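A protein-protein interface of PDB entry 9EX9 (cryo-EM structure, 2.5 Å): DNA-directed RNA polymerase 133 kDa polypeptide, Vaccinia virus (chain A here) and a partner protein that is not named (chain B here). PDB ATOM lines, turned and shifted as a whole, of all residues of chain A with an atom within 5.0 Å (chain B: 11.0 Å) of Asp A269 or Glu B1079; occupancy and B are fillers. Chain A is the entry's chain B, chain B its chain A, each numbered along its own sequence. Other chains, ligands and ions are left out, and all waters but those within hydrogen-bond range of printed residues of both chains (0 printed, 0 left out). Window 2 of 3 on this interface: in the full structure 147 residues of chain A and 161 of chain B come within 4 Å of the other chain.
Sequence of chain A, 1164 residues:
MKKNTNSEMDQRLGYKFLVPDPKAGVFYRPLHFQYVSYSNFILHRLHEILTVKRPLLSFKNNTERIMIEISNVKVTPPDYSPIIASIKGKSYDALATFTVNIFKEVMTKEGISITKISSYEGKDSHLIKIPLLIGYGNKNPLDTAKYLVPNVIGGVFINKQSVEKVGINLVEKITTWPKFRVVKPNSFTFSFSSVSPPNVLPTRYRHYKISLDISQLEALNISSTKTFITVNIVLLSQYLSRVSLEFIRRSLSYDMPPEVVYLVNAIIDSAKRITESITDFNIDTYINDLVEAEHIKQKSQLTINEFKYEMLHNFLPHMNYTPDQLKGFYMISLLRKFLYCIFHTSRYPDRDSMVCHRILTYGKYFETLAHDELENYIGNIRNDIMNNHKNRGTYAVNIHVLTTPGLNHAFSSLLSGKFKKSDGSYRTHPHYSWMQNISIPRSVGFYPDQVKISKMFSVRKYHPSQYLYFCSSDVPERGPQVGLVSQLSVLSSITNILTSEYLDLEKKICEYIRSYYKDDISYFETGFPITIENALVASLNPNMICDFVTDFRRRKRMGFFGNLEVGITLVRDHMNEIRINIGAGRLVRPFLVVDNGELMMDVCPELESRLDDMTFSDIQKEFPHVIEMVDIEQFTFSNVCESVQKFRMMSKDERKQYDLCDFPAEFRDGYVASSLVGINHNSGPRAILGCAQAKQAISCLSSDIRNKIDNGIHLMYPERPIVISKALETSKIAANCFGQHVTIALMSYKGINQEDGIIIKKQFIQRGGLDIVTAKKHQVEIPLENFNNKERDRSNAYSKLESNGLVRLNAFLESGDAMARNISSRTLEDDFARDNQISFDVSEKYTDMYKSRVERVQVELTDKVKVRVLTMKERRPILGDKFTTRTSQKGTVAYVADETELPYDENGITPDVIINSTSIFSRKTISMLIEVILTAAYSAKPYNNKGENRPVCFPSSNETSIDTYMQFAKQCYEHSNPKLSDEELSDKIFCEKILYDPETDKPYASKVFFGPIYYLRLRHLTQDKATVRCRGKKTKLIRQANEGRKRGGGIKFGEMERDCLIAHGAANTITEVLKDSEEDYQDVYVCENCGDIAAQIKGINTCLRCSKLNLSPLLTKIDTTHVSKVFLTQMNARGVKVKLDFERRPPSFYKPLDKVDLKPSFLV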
ATOM      1  N   ARG A 249      22.117  -2.510 -23.329  1.00  0.00           N
ATOM      2  CA  ARG A 249      21.460  -2.700 -24.620  1.00  0.00           C
ATOM      3  C   ARG A 249      22.349  -3.494 -25.567  1.00  0.00           C
ATOM      4  O   ARG A 249      21.913  -4.483 -26.171  1.00  0.00           O
ATOM      5  CB  ARG A 249      21.104  -1.342 -25.230  1.00  0.00           C
ATOM      6  CG  ARG A 249      20.570  -1.414 -26.654  1.00  0.00           C
ATOM      7  CD  ARG A 249      20.474  -0.049 -27.310  1.00  0.00           C
ATOM      8  NE  ARG A 249      19.161   0.562 -27.140  1.00  0.00           N
ATOM      9  CZ  ARG A 249      18.935   1.750 -26.593  1.00  0.00           C
ATOM     10  NH1 ARG A 249      19.919   2.515 -26.154  1.00  0.00           N
ATOM     11  NH2 ARG A 249      17.683   2.187 -26.493  1.00  0.00           N
ATOM     12  N   VAL A 264      14.061  -5.671 -26.658  1.00  0.00           N
ATOM     13  CA  VAL A 264      15.212  -5.166 -25.913  1.00  0.00           C
ATOM     14  C   VAL A 264      15.217  -3.644 -25.913  1.00  0.00           C
ATOM     15  O   VAL A 264      15.382  -3.000 -24.868  1.00  0.00           O
ATOM     16  CB  VAL A 264      16.515  -5.726 -26.504  1.00  0.00           C
ATOM     17  CG1 VAL A 264      17.704  -4.922 -26.023  1.00  0.00           C
ATOM     18  CG2 VAL A 264      16.679  -7.183 -26.136  1.00  0.00           C
ATOM     19  N   ASN A 265      15.051  -3.044 -27.092  1.00  0.00           N
ATOM     20  CA  ASN A 265      15.065  -1.591 -27.189  1.00  0.00           C
ATOM     21  C   ASN A 265      13.927  -0.980 -26.388  1.00  0.00           C
ATOM     22  O   ASN A 265      14.114   0.036 -25.707  1.00  0.00           O
ATOM     23  CB  ASN A 265      14.976  -1.160 -28.651  1.00  0.00           C
ATOM     24  CG  ASN A 265      16.213  -1.519 -29.439  1.00  0.00           C
ATOM     25  OD1 ASN A 265      17.295  -1.668 -28.880  1.00  0.00           O
ATOM     26  ND2 ASN A 265      16.063  -1.650 -30.748  1.00  0.00           N
ATOM     27  N   ALA A 266      12.739  -1.582 -26.452  1.00  0.00           N
ATOM     28  CA  ALA A 266      11.617  -1.047 -25.693  1.00  0.00           C
ATOM     29  C   ALA A 266      11.913  -1.054 -24.200  1.00  0.00           C
ATOM     30  O   ALA A 266      11.666  -0.063 -23.502  1.00  0.00           O
ATOM     31  CB  ALA A 266      10.355  -1.850 -25.994  1.00  0.00           C
ATOM     32  N   ILE A 267      12.464  -2.158 -23.693  1.00  0.00           N
ATOM     33  CA  ILE A 267      12.766  -2.256 -22.266  1.00  0.00           C
ATOM     34  C   ILE A 267      13.794  -1.207 -21.863  1.00  0.00           C
ATOM     35  O   ILE A 267      13.647  -0.522 -20.841  1.00  0.00           O
ATOM     36  CB  ILE A 267      13.254  -3.672 -21.922  1.00  0.00           C
ATOM     37  CG1 ILE A 267      12.090  -4.654 -21.968  1.00  0.00           C
ATOM     38  CG2 ILE A 267      13.926  -3.682 -20.564  1.00  0.00           C
ATOM     39  CD1 ILE A 267      12.526  -6.090 -21.905  1.00  0.00           C
ATOM     40  N   ILE A 268      14.864  -1.077 -22.647  1.00  0.00           N
ATOM     41  CA  ILE A 268      15.919  -0.137 -22.281  1.00  0.00           C
ATOM     42  C   ILE A 268      15.387   1.290 -22.284  1.00  0.00           C
ATOM     43  O   ILE A 268      15.701   2.087 -21.391  1.00  0.00           O
ATOM     44  CB  ILE A 268      17.126  -0.288 -23.221  1.00  0.00           C
ATOM     45  CG1 ILE A 268      17.734  -1.686 -23.095  1.00  0.00           C
ATOM     46  CG2 ILE A 268      18.160   0.772 -22.913  1.00  0.00           C
ATOM     47  CD1 ILE A 268      18.346  -1.980 -21.753  1.00  0.00           C
ATOM     48  N   ASP A 269      14.585   1.643 -23.287  1.00  0.00           N
ATOM     49  CA  ASP A 269      14.056   3.000 -23.336  1.00  0.00           C
ATOM     50  C   ASP A 269      13.081   3.256 -22.195  1.00  0.00           C
ATOM     51  O   ASP A 269      13.026   4.369 -21.663  1.00  0.00           O
ATOM     52  CB  ASP A 269      13.396   3.258 -24.685  1.00  0.00           C
ATOM     53  CG  ASP A 269      14.403   3.349 -25.812  1.00  0.00           C
ATOM     54  OD1 ASP A 269      15.581   3.648 -25.535  1.00  0.00           O
ATOM     55  OD2 ASP A 269      14.017   3.123 -26.975  1.00  0.00           O
ATOM     56  N   SER A 270      12.306   2.247 -21.797  1.00  0.00           N
ATOM     57  CA  SER A 270      11.440   2.420 -20.635  1.00  0.00           C
ATOM     58  C   SER A 270      12.262   2.681 -19.378  1.00  0.00           C
ATOM     59  O   SER A 270      11.915   3.546 -18.561  1.00  0.00           O
ATOM     60  CB  SER A 270      10.554   1.193 -20.453  1.00  0.00           C
ATOM     61  OG  SER A 270       9.650   1.059 -21.533  1.00  0.00           O
ATOM     62  N   ALA A 271      13.357   1.940 -19.204  1.00  0.00           N
ATOM     63  CA  ALA A 271      14.220   2.182 -18.053  1.00  0.00           C
ATOM     64  C   ALA A 271      14.777   3.598 -18.077  1.00  0.00           C
ATOM     65  O   ALA A 271      14.818   4.279 -17.046  1.00  0.00           O
ATOM     66  CB  ALA A 271      15.359   1.167 -18.023  1.00  0.00           C
ATOM     67  N   LYS A 272      15.212   4.059 -19.248  1.00  0.00           N
ATOM     68  CA  LYS A 272      15.741   5.416 -19.340  1.00  0.00           C
ATOM     69  C   LYS A 272      14.668   6.447 -19.009  1.00  0.00           C
ATOM     70  O   LYS A 272      14.946   7.455 -18.348  1.00  0.00           O
ATOM     71  CB  LYS A 272      16.312   5.659 -20.732  1.00  0.00           C
ATOM     72  CG  LYS A 272      17.138   6.921 -20.839  1.00  0.00           C
ATOM     73  CD  LYS A 272      17.682   7.112 -22.242  1.00  0.00           C
ATOM     74  CE  LYS A 272      18.682   6.029 -22.613  1.00  0.00           C
ATOM     75  NZ  LYS A 272      19.286   6.270 -23.949  1.00  0.00           N
ATOM     76  N   ARG A 273      13.435   6.216 -19.463  1.00  0.00           N
ATOM     77  CA  ARG A 273      12.355   7.143 -19.145  1.00  0.00           C
ATOM     78  C   ARG A 273      12.109   7.201 -17.645  1.00  0.00           C
ATOM     79  O   ARG A 273      11.883   8.280 -17.088  1.00  0.00           O
ATOM     80  CB  ARG A 273      11.076   6.737 -19.875  1.00  0.00           C
ATOM     81  CG  ARG A 273       9.911   7.675 -19.621  1.00  0.00           C
ATOM     82  CD  ARG A 273       8.709   7.305 -20.464  1.00  0.00           C
ATOM     83  NE  ARG A 273       7.573   8.182 -20.208  1.00  0.00           N
ATOM     84  CZ  ARG A 273       7.430   9.395 -20.723  1.00  0.00           C
ATOM     85  NH1 ARG A 273       8.349   9.925 -21.514  1.00  0.00           N
ATOM     86  NH2 ARG A 273       6.338  10.097 -20.435  1.00  0.00           N
ATOM     87  N   LEU B1009      13.065  -0.469 -41.623  1.00  0.00           N
ATOM     88  CA  LEU B1009      12.783   0.873 -41.139  1.00  0.00           C
ATOM     89  C   LEU B1009      14.035   1.733 -41.205  1.00  0.00           C
ATOM     90  O   LEU B1009      15.149   1.260 -40.970  1.00  0.00           O
ATOM     91  CB  LEU B1009      12.257   0.848 -39.699  1.00  0.00           C
ATOM     92  CG  LEU B1009      12.024   2.209 -39.036  1.00  0.00           C
ATOM     93  CD1 LEU B1009      10.862   2.133 -38.072  1.00  0.00           C
ATOM     94  CD2 LEU B1009      13.261   2.692 -38.302  1.00  0.00           C
ATOM     95  N   LYS B1011      15.214   6.221 -40.620  1.00  0.00           N
ATOM     96  CA  LYS B1011      14.816   7.535 -40.138  1.00  0.00           C
ATOM     97  C   LYS B1011      15.372   8.602 -41.062  1.00  0.00           C
ATOM     98  O   LYS B1011      16.545   8.547 -41.445  1.00  0.00           O
ATOM     99  CB  LYS B1011      15.307   7.780 -38.711  1.00  0.00           C
ATOM    100  CG  LYS B1011      14.905   9.139 -38.172  1.00  0.00           C
ATOM    101  CD  LYS B1011      15.367   9.348 -36.746  1.00  0.00           C
ATOM    102  CE  LYS B1011      14.794  10.635 -36.178  1.00  0.00           C
ATOM    103  NZ  LYS B1011      15.171  10.834 -34.754  1.00  0.00           N
ATOM    104  N   TYR B1016       9.844   8.923 -40.364  1.00  0.00           N
ATOM    105  CA  TYR B1016      10.344   7.559 -40.372  1.00  0.00           C
ATOM    106  C   TYR B1016       9.740   6.849 -41.570  1.00  0.00           C
ATOM    107  O   TYR B1016       8.531   6.945 -41.802  1.00  0.00           O
ATOM    108  CB  TYR B1016       9.990   6.827 -39.081  1.00  0.00           C
ATOM    109  CG  TYR B1016      10.730   7.342 -37.875  1.00  0.00           C
ATOM    110  CD1 TYR B1016      12.005   6.892 -37.579  1.00  0.00           C
ATOM    111  CD2 TYR B1016      10.153   8.275 -37.031  1.00  0.00           C
ATOM    112  CE1 TYR B1016      12.686   7.355 -36.477  1.00  0.00           C
ATOM    113  CE2 TYR B1016      10.827   8.746 -35.925  1.00  0.00           C
ATOM    114  CZ  TYR B1016      12.093   8.284 -35.654  1.00  0.00           C
ATOM    115  OH  TYR B1016      12.770   8.750 -34.552  1.00  0.00           O
ATOM    116  N   ILE B1050      -0.790   5.463 -31.112  1.00  0.00           N
ATOM    117  CA  ILE B1050       0.611   5.797 -30.896  1.00  0.00           C
ATOM    118  C   ILE B1050       1.238   6.420 -32.131  1.00  0.00           C
ATOM    119  O   ILE B1050       2.460   6.565 -32.193  1.00  0.00           O
ATOM    120  CB  ILE B1050       1.414   4.569 -30.439  1.00  0.00           C
ATOM    121  CG1 ILE B1050       1.559   3.559 -31.574  1.00  0.00           C
ATOM    122  CG2 ILE B1050       0.736   3.915 -29.256  1.00  0.00           C
ATOM    123  CD1 ILE B1050       2.399   2.366 -31.206  1.00  0.00           C
ATOM    124  N   ASN B1073       5.282   9.739 -38.107  1.00  0.00           N
ATOM    125  CA  ASN B1073       5.805  10.509 -36.983  1.00  0.00           C
ATOM    126  C   ASN B1073       4.964  10.162 -35.767  1.00  0.00           C
ATOM    127  O   ASN B1073       3.742  10.346 -35.791  1.00  0.00           O
ATOM    128  CB  ASN B1073       5.766  12.014 -37.253  1.00  0.00           C
ATOM    129  CG  ASN B1073       6.967  12.498 -38.035  1.00  0.00           C
ATOM    130  OD1 ASN B1073       8.044  12.700 -37.476  1.00  0.00           O
ATOM    131  ND2 ASN B1073       6.788  12.692 -39.334  1.00  0.00           N
ATOM    132  N   PHE B1074       5.617   9.669 -34.717  1.00  0.00           N
ATOM    133  CA  PHE B1074       4.945   9.134 -33.543  1.00  0.00           C
ATOM    134  C   PHE B1074       4.670  10.226 -32.515  1.00  0.00           C
ATOM    135  O   PHE B1074       5.184  11.342 -32.596  1.00  0.00           O
ATOM    136  CB  PHE B1074       5.787   8.036 -32.894  1.00  0.00           C
ATOM    137  CG  PHE B1074       6.239   6.979 -33.844  1.00  0.00           C
ATOM    138  CD1 PHE B1074       5.469   5.857 -34.064  1.00  0.00           C
ATOM    139  CD2 PHE B1074       7.440   7.101 -34.513  1.00  0.00           C
ATOM    140  CE1 PHE B1074       5.884   4.882 -34.938  1.00  0.00           C
ATOM    141  CE2 PHE B1074       7.860   6.128 -35.386  1.00  0.00           C
ATOM    142  CZ  PHE B1074       7.081   5.018 -35.598  1.00  0.00           C
ATOM    143  N   VAL B1075       3.851   9.880 -31.528  1.00  0.00           N
ATOM    144  CA  VAL B1075       3.561  10.776 -30.421  1.00  0.00           C
ATOM    145  C   VAL B1075       4.635  10.611 -29.356  1.00  0.00           C
ATOM    146  O   VAL B1075       5.385   9.633 -29.339  1.00  0.00           O
ATOM    147  CB  VAL B1075       2.160  10.519 -29.833  1.00  0.00           C
ATOM    148  CG1 VAL B1075       1.104  10.630 -30.915  1.00  0.00           C
ATOM    149  CG2 VAL B1075       2.105   9.160 -29.161  1.00  0.00           C
ATOM    150  N   GLU B1076       4.712  11.581 -28.454  1.00  0.00           N
ATOM    151  CA  GLU B1076       5.712  11.531 -27.398  1.00  0.00           C
ATOM    152  C   GLU B1076       5.291  10.535 -26.317  1.00  0.00           C
ATOM    153  O   GLU B1076       4.118  10.496 -25.933  1.00  0.00           O
ATOM    154  CB  GLU B1076       5.905  12.913 -26.784  1.00  0.00           C
ATOM    155  CG  GLU B1076       6.417  13.948 -27.763  1.00  0.00           C
ATOM    156  CD  GLU B1076       6.506  15.333 -27.152  1.00  0.00           C
ATOM    157  OE1 GLU B1076       6.061  15.504 -25.997  1.00  0.00           O
ATOM    158  OE2 GLU B1076       7.021  16.250 -27.825  1.00  0.00           O
ATOM    159  N   PRO B1077       6.223   9.719 -25.796  1.00  0.00           N
ATOM    160  CA  PRO B1077       7.659   9.642 -26.112  1.00  0.00           C
ATOM    161  C   PRO B1077       7.912   9.006 -27.472  1.00  0.00           C
ATOM    162  O   PRO B1077       7.118   8.198 -27.939  1.00  0.00           O
ATOM    163  CB  PRO B1077       8.213   8.790 -24.965  1.00  0.00           C
ATOM    164  CG  PRO B1077       7.078   7.898 -24.592  1.00  0.00           C
ATOM    165  CD  PRO B1077       5.843   8.739 -24.765  1.00  0.00           C
ATOM    166  N   GLU B1078       9.019   9.345 -28.128  1.00  0.00           N
ATOM    167  CA  GLU B1078       9.202   8.952 -29.519  1.00  0.00           C
ATOM    168  C   GLU B1078       9.747   7.535 -29.647  1.00  0.00           C
ATOM    169  O   GLU B1078       9.092   6.660 -30.219  1.00  0.00           O
ATOM    170  CB  GLU B1078      10.128   9.944 -30.221  1.00  0.00           C
ATOM    171  CG  GLU B1078      10.313   9.662 -31.695  1.00  0.00           C
ATOM    172  CD  GLU B1078      11.079  10.756 -32.401  1.00  0.00           C
ATOM    173  OE1 GLU B1078      11.468  11.735 -31.732  1.00  0.00           O
ATOM    174  OE2 GLU B1078      11.294  10.638 -33.626  1.00  0.00           O
ATOM    175  N   GLU B1079      10.949   7.286 -29.123  1.00  0.00           N
ATOM    176  CA  GLU B1079      11.614   6.012 -29.389  1.00  0.00           C
ATOM    177  C   GLU B1079      10.897   4.843 -28.725  1.00  0.00           C
ATOM    178  O   GLU B1079      10.873   3.736 -29.277  1.00  0.00           O
ATOM    179  CB  GLU B1079      13.067   6.077 -28.933  1.00  0.00           C
ATOM    180  CG  GLU B1079      13.881   7.120 -29.674  1.00  0.00           C
ATOM    181  CD  GLU B1079      15.356   7.064 -29.337  1.00  0.00           C
ATOM    182  OE1 GLU B1079      15.816   6.018 -28.833  1.00  0.00           O
ATOM    183  OE2 GLU B1079      16.058   8.069 -29.575  1.00  0.00           O
ATOM    184  N   LEU B1080      10.310   5.062 -27.551  1.00  0.00           N
ATOM    185  CA  LEU B1080       9.536   4.005 -26.913  1.00  0.00           C
ATOM    186  C   LEU B1080       8.370   3.581 -27.800  1.00  0.00           C
ATOM    187  O   LEU B1080       8.149   2.384 -28.037  1.00  0.00           O
ATOM    188  CB  LEU B1080       9.051   4.491 -25.547  1.00  0.00           C
ATOM    189  CG  LEU B1080       8.254   3.528 -24.669  1.00  0.00           C
ATOM    190  CD1 LEU B1080       8.358   3.947 -23.218  1.00  0.00           C
ATOM    191  CD2 LEU B1080       6.800   3.483 -25.089  1.00  0.00           C
ATOM    192  N   ASN B1081       7.625   4.557 -28.326  1.00  0.00           N
ATOM    193  CA  ASN B1081       6.516   4.231 -29.212  1.00  0.00           C
ATOM    194  C   ASN B1081       7.003   3.630 -30.521  1.00  0.00           C
ATOM    195  O   ASN B1081       6.329   2.768 -31.089  1.00  0.00           O
ATOM    196  CB  ASN B1081       5.673   5.473 -29.483  1.00  0.00           C
ATOM    197  CG  ASN B1081       4.749   5.808 -28.334  1.00  0.00           C
ATOM    198  OD1 ASN B1081       4.438   4.956 -27.504  1.00  0.00           O
ATOM    199  ND2 ASN B1081       4.296   7.053 -28.282  1.00  0.00           N
ATOM    200  N   LEU B1082       8.162   4.063 -31.015  1.00  0.00           N
ATOM    201  CA  LEU B1082       8.708   3.467 -32.228  1.00  0.00           C
ATOM    202  C   LEU B1082       8.976   1.986 -32.022  1.00  0.00           C
ATOM    203  O   LEU B1082       8.626   1.150 -32.866  1.00  0.00           O
ATOM    204  CB  LEU B1082       9.988   4.197 -32.632  1.00  0.00           C
ATOM    205  CG  LEU B1082      10.599   3.853 -33.991  1.00  0.00           C
ATOM    206  CD1 LEU B1082      11.615   4.903 -34.374  1.00  0.00           C
ATOM    207  CD2 LEU B1082      11.246   2.485 -33.986  1.00  0.00           C
ATOM    208  N   SER B1083       9.604   1.641 -30.898  1.00  0.00           N
ATOM    209  CA  SER B1083       9.879   0.238 -30.619  1.00  0.00           C
ATOM    210  C   SER B1083       8.587  -0.550 -30.472  1.00  0.00           C
ATOM    211  O   SER B1083       8.458  -1.650 -31.022  1.00  0.00           O
ATOM    212  CB  SER B1083      10.732   0.115 -29.361  1.00  0.00           C
ATOM    213  OG  SER B1083      10.151   0.831 -28.287  1.00  0.00           O
ATOM    214  N   LYS B1084       7.608   0.001 -29.756  1.00  0.00           N
ATOM    215  CA  LYS B1084       6.341  -0.709 -29.609  1.00  0.00           C
ATOM    216  C   LYS B1084       5.679  -0.940 -30.963  1.00  0.00           C
ATOM    217  O   LYS B1084       5.147  -2.026 -31.228  1.00  0.00           O
ATOM    218  CB  LYS B1084       5.407   0.069 -28.689  1.00  0.00           C
ATOM    219  CG  LYS B1084       5.828   0.062 -27.236  1.00  0.00           C
ATOM    220  CD  LYS B1084       4.843   0.849 -26.395  1.00  0.00           C
ATOM    221  CE  LYS B1084       5.110   0.694 -24.912  1.00  0.00           C
ATOM    222  NZ  LYS B1084       4.210   1.564 -24.106  1.00  0.00           N
ATOM    223  N   PHE B1085       5.693   0.075 -31.827  1.00  0.00           N
ATOM    224  CA  PHE B1085       5.070  -0.043 -33.139  1.00  0.00           C
ATOM    225  C   PHE B1085       5.750  -1.118 -33.974  1.00  0.00           C
ATOM    226  O   PHE B1085       5.084  -1.965 -34.581  1.00  0.00           O
ATOM    227  CB  PHE B1085       5.124   1.312 -33.843  1.00  0.00           C
ATOM    228  CG  PHE B1085       4.724   1.271 -35.286  1.00  0.00           C
ATOM    229  CD1 PHE B1085       5.660   1.019 -36.269  1.00  0.00           C
ATOM    230  CD2 PHE B1085       3.418   1.509 -35.662  1.00  0.00           C
ATOM    231  CE1 PHE B1085       5.297   0.987 -37.592  1.00  0.00           C
ATOM    232  CE2 PHE B1085       3.053   1.481 -36.985  1.00  0.00           C
ATOM    233  CZ  PHE B1085       3.994   1.221 -37.951  1.00  0.00           C
ATOM    234  N   MET B1086       7.083  -1.089 -34.035  1.00  0.00           N
ATOM    235  CA  MET B1086       7.790  -2.100 -34.812  1.00  0.00           C
ATOM    236  C   MET B1086       7.599  -3.486 -34.220  1.00  0.00           C
ATOM    237  O   MET B1086       7.719  -4.485 -34.936  1.00  0.00           O
ATOM    238  CB  MET B1086       9.278  -1.769 -34.892  1.00  0.00           C
ATOM    239  CG  MET B1086       9.596  -0.559 -35.741  1.00  0.00           C
ATOM    240  SD  MET B1086       9.094  -0.744 -37.460  1.00  0.00           S
ATOM    241  CE  MET B1086      10.089  -2.140 -37.960  1.00  0.00           C
ATOM    242  N   MET B1087       7.316  -3.574 -32.923  1.00  0.00           N
ATOM    243  CA  MET B1087       7.088  -4.876 -32.316  1.00  0.00           C
ATOM    244  C   MET B1087       5.707  -5.418 -32.651  1.00  0.00           C
ATOM    245  O   MET B1087       5.558  -6.615 -32.909  1.00  0.00           O
ATOM    246  CB  MET B1087       7.269  -4.779 -30.805  1.00  0.00           C
ATOM    247  CG  MET B1087       7.162  -6.100 -30.083  1.00  0.00           C
ATOM    248  SD  MET B1087       7.872  -6.035 -28.432  1.00  0.00           S
ATOM    249  CE  MET B1087       7.067  -4.586 -27.769  1.00  0.00           C
ATOM    250  N   VAL B1088       4.686  -4.559 -32.661  1.00  0.00           N
ATOM    251  CA  VAL B1088       3.311  -5.027 -32.830  1.00  0.00           C
ATOM    252  C   VAL B1088       2.831  -5.000 -34.275  1.00  0.00           C
ATOM    253  O   VAL B1088       1.736  -5.516 -34.552  1.00  0.00           O
ATOM    254  CB  VAL B1088       2.322  -4.213 -31.966  1.00  0.00           C
ATOM    255  CG1 VAL B1088       2.701  -4.295 -30.505  1.00  0.00           C
ATOM    256  CG2 VAL B1088       2.260  -2.773 -32.432  1.00  0.00           C
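The backbone carbonyl oxygen (O) of Glu B1079 is in hydrogen-bond range of the side-chain hydroxyl (OG) of Ser B1083 (3.2 Å).
The guanidinium group (NH2) of Arg A249 is in salt-bridge range of the side-chain carboxylate (OD1) of Asp A269 (2.7 Å).
OG of Ser B1083 is in hydrogen-bond range of O of Leu B1080, at 2.5 Å.
The side-chain hydroxyl (OG) of Ser A270 sits at hydrogen-bond distance from the backbone carbonyl oxygen (O) of Ala A266, at 3.0 Å.
The side-chain amide nitrogen (ND2) of Asn B1081 is in hydrogen-bond range of the backbone carbonyl oxygen (O) of Pro B1077 (3.1 Å).
Among the printed residues, merely in contact across the chains: Ala A266 with Ser B1083 (3.5 Å), Ser A270 with Leu B1080 (3.6 Å), Arg A273 with Pro B1077 (3.6 Å) and Asp A269 with Glu B1079 (3.7 Å).
Asp A269 touches just one residue of chain B: Glu B1079.
Glu B1079 touches just one residue of chain A: Asp A269.
Asn A265 touches none of the printed residues of chain B.
Ala A266 touches just one residue of chain B: Ser B1083.
Ile A268 touches none of the printed residues of chain B.
No residue of chain B comes within 4 Å of Ala A271.
No residue of chain B comes within 4 Å of Lys A272.
Of the printed residues of chain A, Leu B1080 touches Ser A270 (3.6 Å).
Printed residues of chain A within 4 Å of Ser B1083: Ala A266 (3.5 Å).
Of the printed residues of chain A, Pro B1077 touches Arg A273.
Of the printed residues of chain B, Arg A273 touches Pro B1077 (3.6 Å).
The nearest residue of chain A that does not touch Glu B1079 is Arg A249 (4.9 Å).
Of the 20 printed residues of chain B, 4 touch a printed residue of chain A.
Hydrophobic or aromatic side chains of chain B that line the printed part of chain A: Pro B1077 and Leu B1080.
Among the printed residues, no Asp or Glu carboxylate lies within 4 Å of a Lys or Arg side-chain nitrogen of the other chain.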
